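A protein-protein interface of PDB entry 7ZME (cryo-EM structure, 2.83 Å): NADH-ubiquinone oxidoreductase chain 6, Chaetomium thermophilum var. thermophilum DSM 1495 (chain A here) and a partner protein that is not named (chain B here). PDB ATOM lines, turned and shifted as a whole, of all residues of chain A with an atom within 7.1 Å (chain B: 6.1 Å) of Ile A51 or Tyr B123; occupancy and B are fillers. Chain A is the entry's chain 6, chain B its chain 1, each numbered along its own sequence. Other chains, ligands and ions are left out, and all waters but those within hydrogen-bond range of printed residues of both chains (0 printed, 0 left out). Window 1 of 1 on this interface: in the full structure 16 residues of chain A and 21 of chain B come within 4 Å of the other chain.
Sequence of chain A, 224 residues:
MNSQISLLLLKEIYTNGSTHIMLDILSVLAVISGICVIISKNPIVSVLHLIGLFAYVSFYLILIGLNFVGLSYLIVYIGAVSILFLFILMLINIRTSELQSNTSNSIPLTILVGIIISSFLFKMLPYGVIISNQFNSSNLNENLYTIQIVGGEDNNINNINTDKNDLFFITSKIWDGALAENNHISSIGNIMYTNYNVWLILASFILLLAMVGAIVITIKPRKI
CA of Leu A48 touches OH of Tyr B123, 3.4 Å away.
Leu A48 touches Leu B127 (CD1 to CD2, 3.8 Å).
Tyr B123 touches Ile A51.
CD1 of Ile A78 touches OG of Ser B119 (3.2 Å).
CD1 of Ile A78 touches CD2 of Leu B120, at 3.5 Å.
Phe A85 touches Leu B126.
Ile A44 touches none of the printed residues of chain B.
Printed residues of chain B within 4 Å of Ile A51: Tyr B123.
Ala B121 touches none of the printed residues of chain A.
Tyr B123 touches just these residues of chain A: Leu A48 (3.4 Å) and Ile A51 (3.7 Å).
Of the printed residues of chain A, Leu B126 touches Phe A85 (3.5 Å).
Printed residues of chain A within 4 Å of Leu B127: Leu A48.
The nearest residue of chain A that does not touch Tyr B123 is Val A47 (4.1 Å).
The nearest printed residue of chain B that does not touch Leu A48 is Ile B84 (4.8 Å).
Among the printed residues, 6 pairs touch across the chains.
Among the printed residues, no Asp or Glu carboxylate lies within 4 Å of a Lys or Arg side-chain nitrogen of the other chain.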
ATOM      1  N   SER A  33      23.719 -37.039  15.325  1.00  0.00           N
ATOM      2  CA  SER A  33      22.895 -35.868  15.595  1.00  0.00           C
ATOM      3  C   SER A  33      22.305 -35.289  14.318  1.00  0.00           C
ATOM      4  O   SER A  33      21.215 -34.711  14.353  1.00  0.00           O
ATOM      5  CB  SER A  33      23.713 -34.812  16.333  1.00  0.00           C
ATOM      6  OG  SER A  33      24.677 -34.228  15.479  1.00  0.00           O
ATOM      7  N   VAL A  37      18.055 -34.747  13.549  1.00  0.00           N
ATOM      8  CA  VAL A  37      17.456 -33.423  13.204  1.00  0.00           C
ATOM      9  C   VAL A  37      16.227 -33.627  12.311  1.00  0.00           C
ATOM     10  O   VAL A  37      15.269 -32.858  12.445  1.00  0.00           O
ATOM     11  CB  VAL A  37      18.485 -32.509  12.511  1.00  0.00           C
ATOM     12  CG1 VAL A  37      17.859 -31.230  11.981  1.00  0.00           C
ATOM     13  CG2 VAL A  37      19.661 -32.179  13.408  1.00  0.00           C
ATOM     14  N   ILE A  44      11.315 -28.792  18.306  1.00  0.00           N
ATOM     15  CA  ILE A  44      12.311 -28.286  19.300  1.00  0.00           C
ATOM     16  C   ILE A  44      13.405 -29.331  19.550  1.00  0.00           C
ATOM     17  O   ILE A  44      14.576 -28.949  19.673  1.00  0.00           O
ATOM     18  CB  ILE A  44      11.622 -27.783  20.583  1.00  0.00           C
ATOM     19  CG1 ILE A  44      10.637 -26.653  20.279  1.00  0.00           C
ATOM     20  CG2 ILE A  44      12.640 -27.373  21.629  1.00  0.00           C
ATOM     21  CD1 ILE A  44      11.273 -25.410  19.711  1.00  0.00           C
ATOM     22  N   VAL A  45      13.035 -30.604  19.634  1.00  0.00           N
ATOM     23  CA  VAL A  45      14.046 -31.682  19.812  1.00  0.00           C
ATOM     24  C   VAL A  45      14.939 -31.697  18.567  1.00  0.00           C
ATOM     25  O   VAL A  45      16.152 -31.894  18.711  1.00  0.00           O
ATOM     26  CB  VAL A  45      13.371 -33.034  20.103  1.00  0.00           C
ATOM     27  CG1 VAL A  45      14.364 -34.186  20.088  1.00  0.00           C
ATOM     28  CG2 VAL A  45      12.618 -32.999  21.421  1.00  0.00           C
ATOM     29  N   SER A  46      14.563 -31.466  17.441  1.00  0.00           N
ATOM     30  CA  SER A  46      15.396 -31.532  16.216  1.00  0.00           C
ATOM     31  C   SER A  46      16.254 -30.271  16.078  1.00  0.00           C
ATOM     32  O   SER A  46      17.278 -30.343  15.387  1.00  0.00           O
ATOM     33  CB  SER A  46      14.478 -31.703  15.037  1.00  0.00           C
ATOM     34  OG  SER A  46      14.031 -30.456  14.540  1.00  0.00           O
ATOM     35  N   VAL A  47      15.698 -29.080  16.628  1.00  0.00           N
ATOM     36  CA  VAL A  47      16.567 -27.868  16.641  1.00  0.00           C
ATOM     37  C   VAL A  47      17.618 -28.012  17.743  1.00  0.00           C
ATOM     38  O   VAL A  47      18.660 -27.348  17.649  1.00  0.00           O
ATOM     39  CB  VAL A  47      15.763 -26.549  16.707  1.00  0.00           C
ATOM     40  CG1 VAL A  47      15.387 -26.149  18.125  1.00  0.00           C
ATOM     41  CG2 VAL A  47      16.465 -25.406  15.995  1.00  0.00           C
ATOM     42  N   LEU A  48      17.376 -28.888  18.719  1.00  0.00           N
ATOM     43  CA  LEU A  48      18.388 -29.103  19.774  1.00  0.00           C
ATOM     44  C   LEU A  48      19.421 -30.047  19.180  1.00  0.00           C
ATOM     45  O   LEU A  48      20.618 -29.860  19.435  1.00  0.00           O
ATOM     46  CB  LEU A  48      17.722 -29.726  21.002  1.00  0.00           C
ATOM     47  CG  LEU A  48      18.670 -30.334  22.031  1.00  0.00           C
ATOM     48  CD1 LEU A  48      19.097 -29.302  23.059  1.00  0.00           C
ATOM     49  CD2 LEU A  48      18.023 -31.527  22.710  1.00  0.00           C
ATOM     50  N   HIS A  49      18.961 -31.037  18.419  1.00  0.00           N
ATOM     51  CA  HIS A  49      19.956 -31.841  17.729  1.00  0.00           C
ATOM     52  C   HIS A  49      20.720 -31.027  16.701  1.00  0.00           C
ATOM     53  O   HIS A  49      21.837 -31.400  16.335  1.00  0.00           O
ATOM     54  CB  HIS A  49      19.288 -33.040  17.059  1.00  0.00           C
ATOM     55  CG  HIS A  49      19.010 -34.176  17.991  1.00  0.00           C
ATOM     56  ND1 HIS A  49      19.964 -35.110  18.329  1.00  0.00           N
ATOM     57  CD2 HIS A  49      17.885 -34.531  18.653  1.00  0.00           C
ATOM     58  CE1 HIS A  49      19.438 -35.988  19.164  1.00  0.00           C
ATOM     59  NE2 HIS A  49      18.177 -35.662  19.374  1.00  0.00           N
ATOM     60  N   LEU A  50      20.136 -29.927  16.227  1.00  0.00           N
ATOM     61  CA  LEU A  50      20.817 -29.077  15.259  1.00  0.00           C
ATOM     62  C   LEU A  50      21.972 -28.324  15.906  1.00  0.00           C
ATOM     63  O   LEU A  50      23.078 -28.284  15.360  1.00  0.00           O
ATOM     64  CB  LEU A  50      19.820 -28.108  14.630  1.00  0.00           C
ATOM     65  CG  LEU A  50      20.347 -27.166  13.554  1.00  0.00           C
ATOM     66  CD1 LEU A  50      20.612 -27.924  12.261  1.00  0.00           C
ATOM     67  CD2 LEU A  50      19.356 -26.061  13.330  1.00  0.00           C
ATOM     68  N   ILE A  51      21.735 -27.718  17.073  1.00  0.00           N
ATOM     69  CA  ILE A  51      22.813 -27.010  17.753  1.00  0.00           C
ATOM     70  C   ILE A  51      23.878 -27.991  18.217  1.00  0.00           C
ATOM     71  O   ILE A  51      25.073 -27.672  18.204  1.00  0.00           O
ATOM     72  CB  ILE A  51      22.272 -26.146  18.912  1.00  0.00           C
ATOM     73  CG1 ILE A  51      23.402 -25.343  19.559  1.00  0.00           C
ATOM     74  CG2 ILE A  51      21.571 -26.982  19.953  1.00  0.00           C
ATOM     75  CD1 ILE A  51      24.047 -24.339  18.632  1.00  0.00           C
ATOM     76  N   GLY A  52      23.477 -29.194  18.622  1.00  0.00           N
ATOM     77  CA  GLY A  52      24.458 -30.223  18.909  1.00  0.00           C
ATOM     78  C   GLY A  52      25.305 -30.552  17.698  1.00  0.00           C
ATOM     79  O   GLY A  52      26.531 -30.616  17.788  1.00  0.00           O
ATOM     80  N   LEU A  53      24.665 -30.709  16.537  1.00  0.00           N
ATOM     81  CA  LEU A  53      25.381 -31.067  15.316  1.00  0.00           C
ATOM     82  C   LEU A  53      26.427 -30.018  14.968  1.00  0.00           C
ATOM     83  O   LEU A  53      27.550 -30.349  14.576  1.00  0.00           O
ATOM     84  CB  LEU A  53      24.384 -31.247  14.171  1.00  0.00           C
ATOM     85  CG  LEU A  53      24.860 -31.199  12.717  1.00  0.00           C
ATOM     86  CD1 LEU A  53      25.857 -32.302  12.410  1.00  0.00           C
ATOM     87  CD2 LEU A  53      23.672 -31.284  11.785  1.00  0.00           C
ATOM     88  N   PHE A  54      26.073 -28.742  15.106  1.00  0.00           N
ATOM     89  CA  PHE A  54      27.047 -27.685  14.874  1.00  0.00           C
ATOM     90  C   PHE A  54      28.151 -27.709  15.924  1.00  0.00           C
ATOM     91  O   PHE A  54      29.262 -27.237  15.666  1.00  0.00           O
ATOM     92  CB  PHE A  54      26.350 -26.325  14.865  1.00  0.00           C
ATOM     93  CG  PHE A  54      25.615 -26.028  13.592  1.00  0.00           C
ATOM     94  CD1 PHE A  54      26.279 -25.529  12.494  1.00  0.00           C
ATOM     95  CD2 PHE A  54      24.254 -26.232  13.502  1.00  0.00           C
ATOM     96  CE1 PHE A  54      25.606 -25.253  11.326  1.00  0.00           C
ATOM     97  CE2 PHE A  54      23.573 -25.955  12.337  1.00  0.00           C
ATOM     98  CZ  PHE A  54      24.250 -25.467  11.248  1.00  0.00           C
ATOM     99  N   ALA A  55      27.864 -28.249  17.109  1.00  0.00           N
ATOM    100  CA  ALA A  55      28.856 -28.274  18.177  1.00  0.00           C
ATOM    101  C   ALA A  55      29.934 -29.322  17.932  1.00  0.00           C
ATOM    102  O   ALA A  55      31.120 -29.041  18.135  1.00  0.00           O
ATOM    103  CB  ALA A  55      28.176 -28.510  19.523  1.00  0.00           C
ATOM    104  N   TYR A  56      29.560 -30.530  17.498  1.00  0.00           N
ATOM    105  CA  TYR A  56      30.586 -31.537  17.243  1.00  0.00           C
ATOM    106  C   TYR A  56      31.443 -31.166  16.046  1.00  0.00           C
ATOM    107  O   TYR A  56      32.625 -31.524  15.999  1.00  0.00           O
ATOM    108  CB  TYR A  56      29.983 -32.927  17.024  1.00  0.00           C
ATOM    109  CG  TYR A  56      28.948 -33.357  18.031  1.00  0.00           C
ATOM    110  CD1 TYR A  56      29.321 -33.861  19.266  1.00  0.00           C
ATOM    111  CD2 TYR A  56      27.598 -33.248  17.754  1.00  0.00           C
ATOM    112  CE1 TYR A  56      28.377 -34.250  20.189  1.00  0.00           C
ATOM    113  CE2 TYR A  56      26.650 -33.634  18.668  1.00  0.00           C
ATOM    114  CZ  TYR A  56      27.044 -34.134  19.884  1.00  0.00           C
ATOM    115  OH  TYR A  56      26.096 -34.517  20.799  1.00  0.00           O
ATOM    116  N   TYR A  73      32.166 -20.411  14.105  1.00  0.00           N
ATOM    117  CA  TYR A  73      31.001 -21.232  13.696  1.00  0.00           C
ATOM    118  C   TYR A  73      30.051 -21.355  14.876  1.00  0.00           C
ATOM    119  O   TYR A  73      28.866 -21.083  14.728  1.00  0.00           O
ATOM    120  CB  TYR A  73      31.443 -22.649  13.319  1.00  0.00           C
ATOM    121  CG  TYR A  73      30.904 -23.141  12.003  1.00  0.00           C
ATOM    122  CD1 TYR A  73      31.702 -23.167  10.877  1.00  0.00           C
ATOM    123  CD2 TYR A  73      29.591 -23.554  11.879  1.00  0.00           C
ATOM    124  CE1 TYR A  73      31.211 -23.599   9.658  1.00  0.00           C
ATOM    125  CE2 TYR A  73      29.084 -23.992  10.668  1.00  0.00           C
ATOM    126  CZ  TYR A  73      29.900 -24.020   9.553  1.00  0.00           C
ATOM    127  OH  TYR A  73      29.414 -24.455   8.358  1.00  0.00           O
ATOM    128  N   LEU A  74      30.581 -21.760  16.019  1.00  0.00           N
ATOM    129  CA  LEU A  74      29.739 -21.968  17.224  1.00  0.00           C
ATOM    130  C   LEU A  74      29.050 -20.652  17.583  1.00  0.00           C
ATOM    131  O   LEU A  74      27.826 -20.653  17.635  1.00  0.00           O
ATOM    132  CB  LEU A  74      30.656 -22.437  18.361  1.00  0.00           C
ATOM    133  CG  LEU A  74      30.028 -23.292  19.455  1.00  0.00           C
ATOM    134  CD1 LEU A  74      29.407 -24.552  18.873  1.00  0.00           C
ATOM    135  CD2 LEU A  74      31.066 -23.645  20.505  1.00  0.00           C
ATOM    136  N   TYR A  77      26.178 -19.686  15.076  1.00  0.00           N
ATOM    137  CA  TYR A  77      25.026 -20.618  15.017  1.00  0.00           C
ATOM    138  C   TYR A  77      24.272 -20.751  16.336  1.00  0.00           C
ATOM    139  O   TYR A  77      23.103 -21.090  16.281  1.00  0.00           O
ATOM    140  CB  TYR A  77      25.449 -21.919  14.332  1.00  0.00           C
ATOM    141  CG  TYR A  77      25.638 -21.688  12.858  1.00  0.00           C
ATOM    142  CD1 TYR A  77      24.548 -21.475  12.041  1.00  0.00           C
ATOM    143  CD2 TYR A  77      26.898 -21.576  12.302  1.00  0.00           C
ATOM    144  CE1 TYR A  77      24.705 -21.199  10.697  1.00  0.00           C
ATOM    145  CE2 TYR A  77      27.072 -21.313  10.955  1.00  0.00           C
ATOM    146  CZ  TYR A  77      25.969 -21.132  10.146  1.00  0.00           C
ATOM    147  OH  TYR A  77      26.116 -20.875   8.814  1.00  0.00           O
ATOM    148  N   ILE A  78      24.910 -20.504  17.470  1.00  0.00           N
ATOM    149  CA  ILE A  78      24.152 -20.540  18.713  1.00  0.00           C
ATOM    150  C   ILE A  78      23.068 -19.470  18.700  1.00  0.00           C
ATOM    151  O   ILE A  78      21.925 -19.718  19.099  1.00  0.00           O
ATOM    152  CB  ILE A  78      25.090 -20.393  19.925  1.00  0.00           C
ATOM    153  CG1 ILE A  78      26.068 -21.564  19.982  1.00  0.00           C
ATOM    154  CG2 ILE A  78      24.290 -20.335  21.216  1.00  0.00           C
ATOM    155  CD1 ILE A  78      27.401 -21.226  20.632  1.00  0.00           C
ATOM    156  N   GLY A  79      23.408 -18.267  18.234  1.00  0.00           N
ATOM    157  CA  GLY A  79      22.392 -17.247  18.039  1.00  0.00           C
ATOM    158  C   GLY A  79      21.423 -17.591  16.925  1.00  0.00           C
ATOM    159  O   GLY A  79      20.230 -17.295  17.012  1.00  0.00           O
ATOM    160  N   ALA A  80      21.925 -18.213  15.857  1.00  0.00           N
ATOM    161  CA  ALA A  80      21.067 -18.587  14.737  1.00  0.00           C
ATOM    162  C   ALA A  80      20.076 -19.675  15.126  1.00  0.00           C
ATOM    163  O   ALA A  80      18.905 -19.624  14.734  1.00  0.00           O
ATOM    164  CB  ALA A  80      21.921 -19.038  13.552  1.00  0.00           C
ATOM    165  N   VAL A  81      20.527 -20.680  15.883  1.00  0.00           N
ATOM    166  CA  VAL A  81      19.624 -21.727  16.352  1.00  0.00           C
ATOM    167  C   VAL A  81      18.644 -21.177  17.377  1.00  0.00           C
ATOM    168  O   VAL A  81      17.494 -21.624  17.445  1.00  0.00           O
ATOM    169  CB  VAL A  81      20.432 -22.920  16.900  1.00  0.00           C
ATOM    170  CG1 VAL A  81      19.519 -24.005  17.403  1.00  0.00           C
ATOM    171  CG2 VAL A  81      21.292 -23.506  15.796  1.00  0.00           C
ATOM    172  N   SER A  82      19.070 -20.205  18.185  1.00  0.00           N
ATOM    173  CA  SER A  82      18.161 -19.583  19.140  1.00  0.00           C
ATOM    174  C   SER A  82      17.019 -18.866  18.433  1.00  0.00           C
ATOM    175  O   SER A  82      15.860 -18.964  18.849  1.00  0.00           O
ATOM    176  CB  SER A  82      18.930 -18.609  20.028  1.00  0.00           C
ATOM    177  OG  SER A  82      20.146 -19.179  20.463  1.00  0.00           O
ATOM    178  N   PHE A  85      14.825 -21.500  16.876  1.00  0.00           N
ATOM    179  CA  PHE A  85      13.949 -21.871  17.982  1.00  0.00           C
ATOM    180  C   PHE A  85      12.813 -20.868  18.141  1.00  0.00           C
ATOM    181  O   PHE A  85      11.649 -21.253  18.299  1.00  0.00           O
ATOM    182  CB  PHE A  85      14.788 -21.958  19.263  1.00  0.00           C
ATOM    183  CG  PHE A  85      14.061 -22.505  20.467  1.00  0.00           C
ATOM    184  CD1 PHE A  85      13.053 -21.786  21.088  1.00  0.00           C
ATOM    185  CD2 PHE A  85      14.432 -23.716  21.013  1.00  0.00           C
ATOM    186  CE1 PHE A  85      12.408 -22.283  22.195  1.00  0.00           C
ATOM    187  CE2 PHE A  85      13.791 -24.210  22.124  1.00  0.00           C
ATOM    188  CZ  PHE A  85      12.777 -23.492  22.713  1.00  0.00           C
ATOM    189  N   GLY B  81      18.610 -28.679  30.095  1.00  0.00           N
ATOM    190  CA  GLY B  81      18.820 -27.251  30.063  1.00  0.00           C
ATOM    191  C   GLY B  81      19.647 -26.725  31.217  1.00  0.00           C
ATOM    192  O   GLY B  81      20.645 -26.027  31.018  1.00  0.00           O
ATOM    193  N   ILE B  84      23.226 -27.904  30.824  1.00  0.00           N
ATOM    194  CA  ILE B  84      23.940 -27.097  29.837  1.00  0.00           C
ATOM    195  C   ILE B  84      24.312 -25.743  30.421  1.00  0.00           C
ATOM    196  O   ILE B  84      25.442 -25.270  30.261  1.00  0.00           O
ATOM    197  CB  ILE B  84      23.095 -26.947  28.556  1.00  0.00           C
ATOM    198  CG1 ILE B  84      22.989 -28.282  27.824  1.00  0.00           C
ATOM    199  CG2 ILE B  84      23.664 -25.874  27.655  1.00  0.00           C
ATOM    200  CD1 ILE B  84      21.971 -28.279  26.709  1.00  0.00           C
ATOM    201  N   THR B  85      23.372 -25.102  31.114  1.00  0.00           N
ATOM    202  CA  THR B  85      23.633 -23.779  31.665  1.00  0.00           C
ATOM    203  C   THR B  85      24.744 -23.822  32.704  1.00  0.00           C
ATOM    204  O   THR B  85      25.592 -22.925  32.749  1.00  0.00           O
ATOM    205  CB  THR B  85      22.348 -23.202  32.263  1.00  0.00           C
ATOM    206  OG1 THR B  85      21.268 -23.409  31.348  1.00  0.00           O
ATOM    207  CG2 THR B  85      22.495 -21.717  32.524  1.00  0.00           C
ATOM    208  N   SER B 118      29.391 -18.503  26.928  1.00  0.00           N
ATOM    209  CA  SER B 118      28.302 -17.740  27.523  1.00  0.00           C
ATOM    210  C   SER B 118      27.021 -17.880  26.708  1.00  0.00           C
ATOM    211  O   SER B 118      25.922 -17.935  27.271  1.00  0.00           O
ATOM    212  CB  SER B 118      28.701 -16.271  27.658  1.00  0.00           C
ATOM    213  OG  SER B 118      28.810 -15.650  26.391  1.00  0.00           O
ATOM    214  N   SER B 119      27.145 -17.940  25.383  1.00  0.00           N
ATOM    215  CA  SER B 119      25.975 -18.083  24.529  1.00  0.00           C
ATOM    216  C   SER B 119      25.329 -19.457  24.656  1.00  0.00           C
ATOM    217  O   SER B 119      24.101 -19.565  24.575  1.00  0.00           O
ATOM    218  CB  SER B 119      26.359 -17.810  23.075  1.00  0.00           C
ATOM    219  OG  SER B 119      27.313 -18.750  22.621  1.00  0.00           O
ATOM    220  N   LEU B 120      26.128 -20.512  24.832  1.00  0.00           N
ATOM    221  CA  LEU B 120      25.559 -21.835  25.075  1.00  0.00           C
ATOM    222  C   LEU B 120      24.776 -21.885  26.378  1.00  0.00           C
ATOM    223  O   LEU B 120      23.679 -22.451  26.428  1.00  0.00           O
ATOM    224  CB  LEU B 120      26.663 -22.890  25.070  1.00  0.00           C
ATOM    225  CG  LEU B 120      27.336 -23.099  23.724  1.00  0.00           C
ATOM    226  CD1 LEU B 120      28.506 -24.044  23.832  1.00  0.00           C
ATOM    227  CD2 LEU B 120      26.291 -23.704  22.821  1.00  0.00           C
ATOM    228  N   ALA B 121      25.323 -21.303  27.448  1.00  0.00           N
ATOM    229  CA  ALA B 121      24.645 -21.349  28.737  1.00  0.00           C
ATOM    230  C   ALA B 121      23.295 -20.645  28.685  1.00  0.00           C
ATOM    231  O   ALA B 121      22.358 -21.047  29.383  1.00  0.00           O
ATOM    232  CB  ALA B 121      25.533 -20.737  29.818  1.00  0.00           C
ATOM    233  N   THR B 122      23.173 -19.602  27.863  1.00  0.00           N
ATOM    234  CA  THR B 122      21.887 -18.937  27.692  1.00  0.00           C
ATOM    235  C   THR B 122      20.874 -19.861  27.029  1.00  0.00           C
ATOM    236  O   THR B 122      19.688 -19.843  27.374  1.00  0.00           O
ATOM    237  CB  THR B 122      22.065 -17.660  26.873  1.00  0.00           C
ATOM    238  OG1 THR B 122      23.157 -16.902  27.408  1.00  0.00           O
ATOM    239  CG2 THR B 122      20.806 -16.815  26.916  1.00  0.00           C
ATOM    240  N   TYR B 123      21.326 -20.679  26.078  1.00  0.00           N
ATOM    241  CA  TYR B 123      20.418 -21.572  25.370  1.00  0.00           C
ATOM    242  C   TYR B 123      19.839 -22.637  26.294  1.00  0.00           C
ATOM    243  O   TYR B 123      18.742 -23.145  26.038  1.00  0.00           O
ATOM    244  CB  TYR B 123      21.145 -22.209  24.188  1.00  0.00           C
ATOM    245  CG  TYR B 123      20.347 -23.264  23.471  1.00  0.00           C
ATOM    246  CD1 TYR B 123      19.281 -22.918  22.655  1.00  0.00           C
ATOM    247  CD2 TYR B 123      20.657 -24.605  23.609  1.00  0.00           C
ATOM    248  CE1 TYR B 123      18.545 -23.879  21.999  1.00  0.00           C
ATOM    249  CE2 TYR B 123      19.928 -25.573  22.957  1.00  0.00           C
ATOM    250  CZ  TYR B 123      18.874 -25.206  22.154  1.00  0.00           C
ATOM    251  OH  TYR B 123      18.146 -26.171  21.502  1.00  0.00           O
ATOM    252  N   GLY B 124      20.551 -22.987  27.365  1.00  0.00           N
ATOM    253  CA  GLY B 124      19.980 -23.883  28.353  1.00  0.00           C
ATOM    254  C   GLY B 124      18.792 -23.276  29.076  1.00  0.00           C
ATOM    255  O   GLY B 124      17.824 -23.972  29.390  1.00  0.00           O
ATOM    256  N   ILE B 125      18.852 -21.974  29.357  1.00  0.00           N
ATOM    257  CA  ILE B 125      17.719 -21.292  29.976  1.00  0.00           C
ATOM    258  C   ILE B 125      16.510 -21.317  29.052  1.00  0.00           C
ATOM    259  O   ILE B 125      15.383 -21.581  29.486  1.00  0.00           O
ATOM    260  CB  ILE B 125      18.112 -19.854  30.360  1.00  0.00           C
ATOM    261  CG1 ILE B 125      19.082 -19.865  31.541  1.00  0.00           C
ATOM    262  CG2 ILE B 125      16.879 -19.020  30.677  1.00  0.00           C
ATOM    263  CD1 ILE B 125      19.820 -18.572  31.726  1.00  0.00           C
ATOM    264  N   LEU B 126      16.726 -21.045  27.765  1.00  0.00           N
ATOM    265  CA  LEU B 126      15.638 -21.103  26.793  1.00  0.00           C
ATOM    266  C   LEU B 126      15.031 -22.497  26.719  1.00  0.00           C
ATOM    267  O   LEU B 126      13.806 -22.649  26.686  1.00  0.00           O
ATOM    268  CB  LEU B 126      16.152 -20.673  25.419  1.00  0.00           C
ATOM    269  CG  LEU B 126      15.214 -20.796  24.219  1.00  0.00           C
ATOM    270  CD1 LEU B 126      13.878 -20.117  24.490  1.00  0.00           C
ATOM    271  CD2 LEU B 126      15.874 -20.220  22.978  1.00  0.00           C
ATOM    272  N   LEU B 127      15.876 -23.527  26.688  1.00  0.00           N
ATOM    273  CA  LEU B 127      15.378 -24.891  26.569  1.00  0.00           C
ATOM    274  C   LEU B 127      14.635 -25.319  27.826  1.00  0.00           C
ATOM    275  O   LEU B 127      13.557 -25.916  27.748  1.00  0.00           O
ATOM    276  CB  LEU B 127      16.538 -25.844  26.272  1.00  0.00           C
ATOM    277  CG  LEU B 127      16.154 -27.241  25.785  1.00  0.00           C
ATOM    278  CD1 LEU B 127      15.961 -27.255  24.286  1.00  0.00           C
ATOM    279  CD2 LEU B 127      17.196 -28.261  26.205  1.00  0.00           C
ATOM    280  N   ALA B 128      15.198 -25.023  28.997  1.00  0.00           N
ATOM    281  CA  ALA B 128      14.574 -25.447  30.246  1.00  0.00           C
ATOM    282  C   ALA B 128      13.229 -24.767  30.459  1.00  0.00           C
ATOM    283  O   ALA B 128      12.275 -25.403  30.920  1.00  0.00           O
ATOM    284  CB  ALA B 128      15.508 -25.172  31.421  1.00  0.00           C
ATOM    285  N   LEU B 148      19.020 -11.829  25.028  1.00  0.00           N
ATOM    286  CA  LEU B 148      20.285 -12.182  24.333  1.00  0.00           C
ATOM    287  C   LEU B 148      20.384 -11.412  23.025  1.00  0.00           C
ATOM    288  O   LEU B 148      21.477 -10.952  22.705  1.00  0.00           O
ATOM    289  CB  LEU B 148      20.431 -13.699  24.159  1.00  0.00           C
ATOM    290  CG  LEU B 148      19.796 -14.364  22.936  1.00  0.00           C
ATOM    291  CD1 LEU B 148      20.788 -14.470  21.789  1.00  0.00           C
ATOM    292  CD2 LEU B 148      19.290 -15.749  23.298  1.00  0.00           C
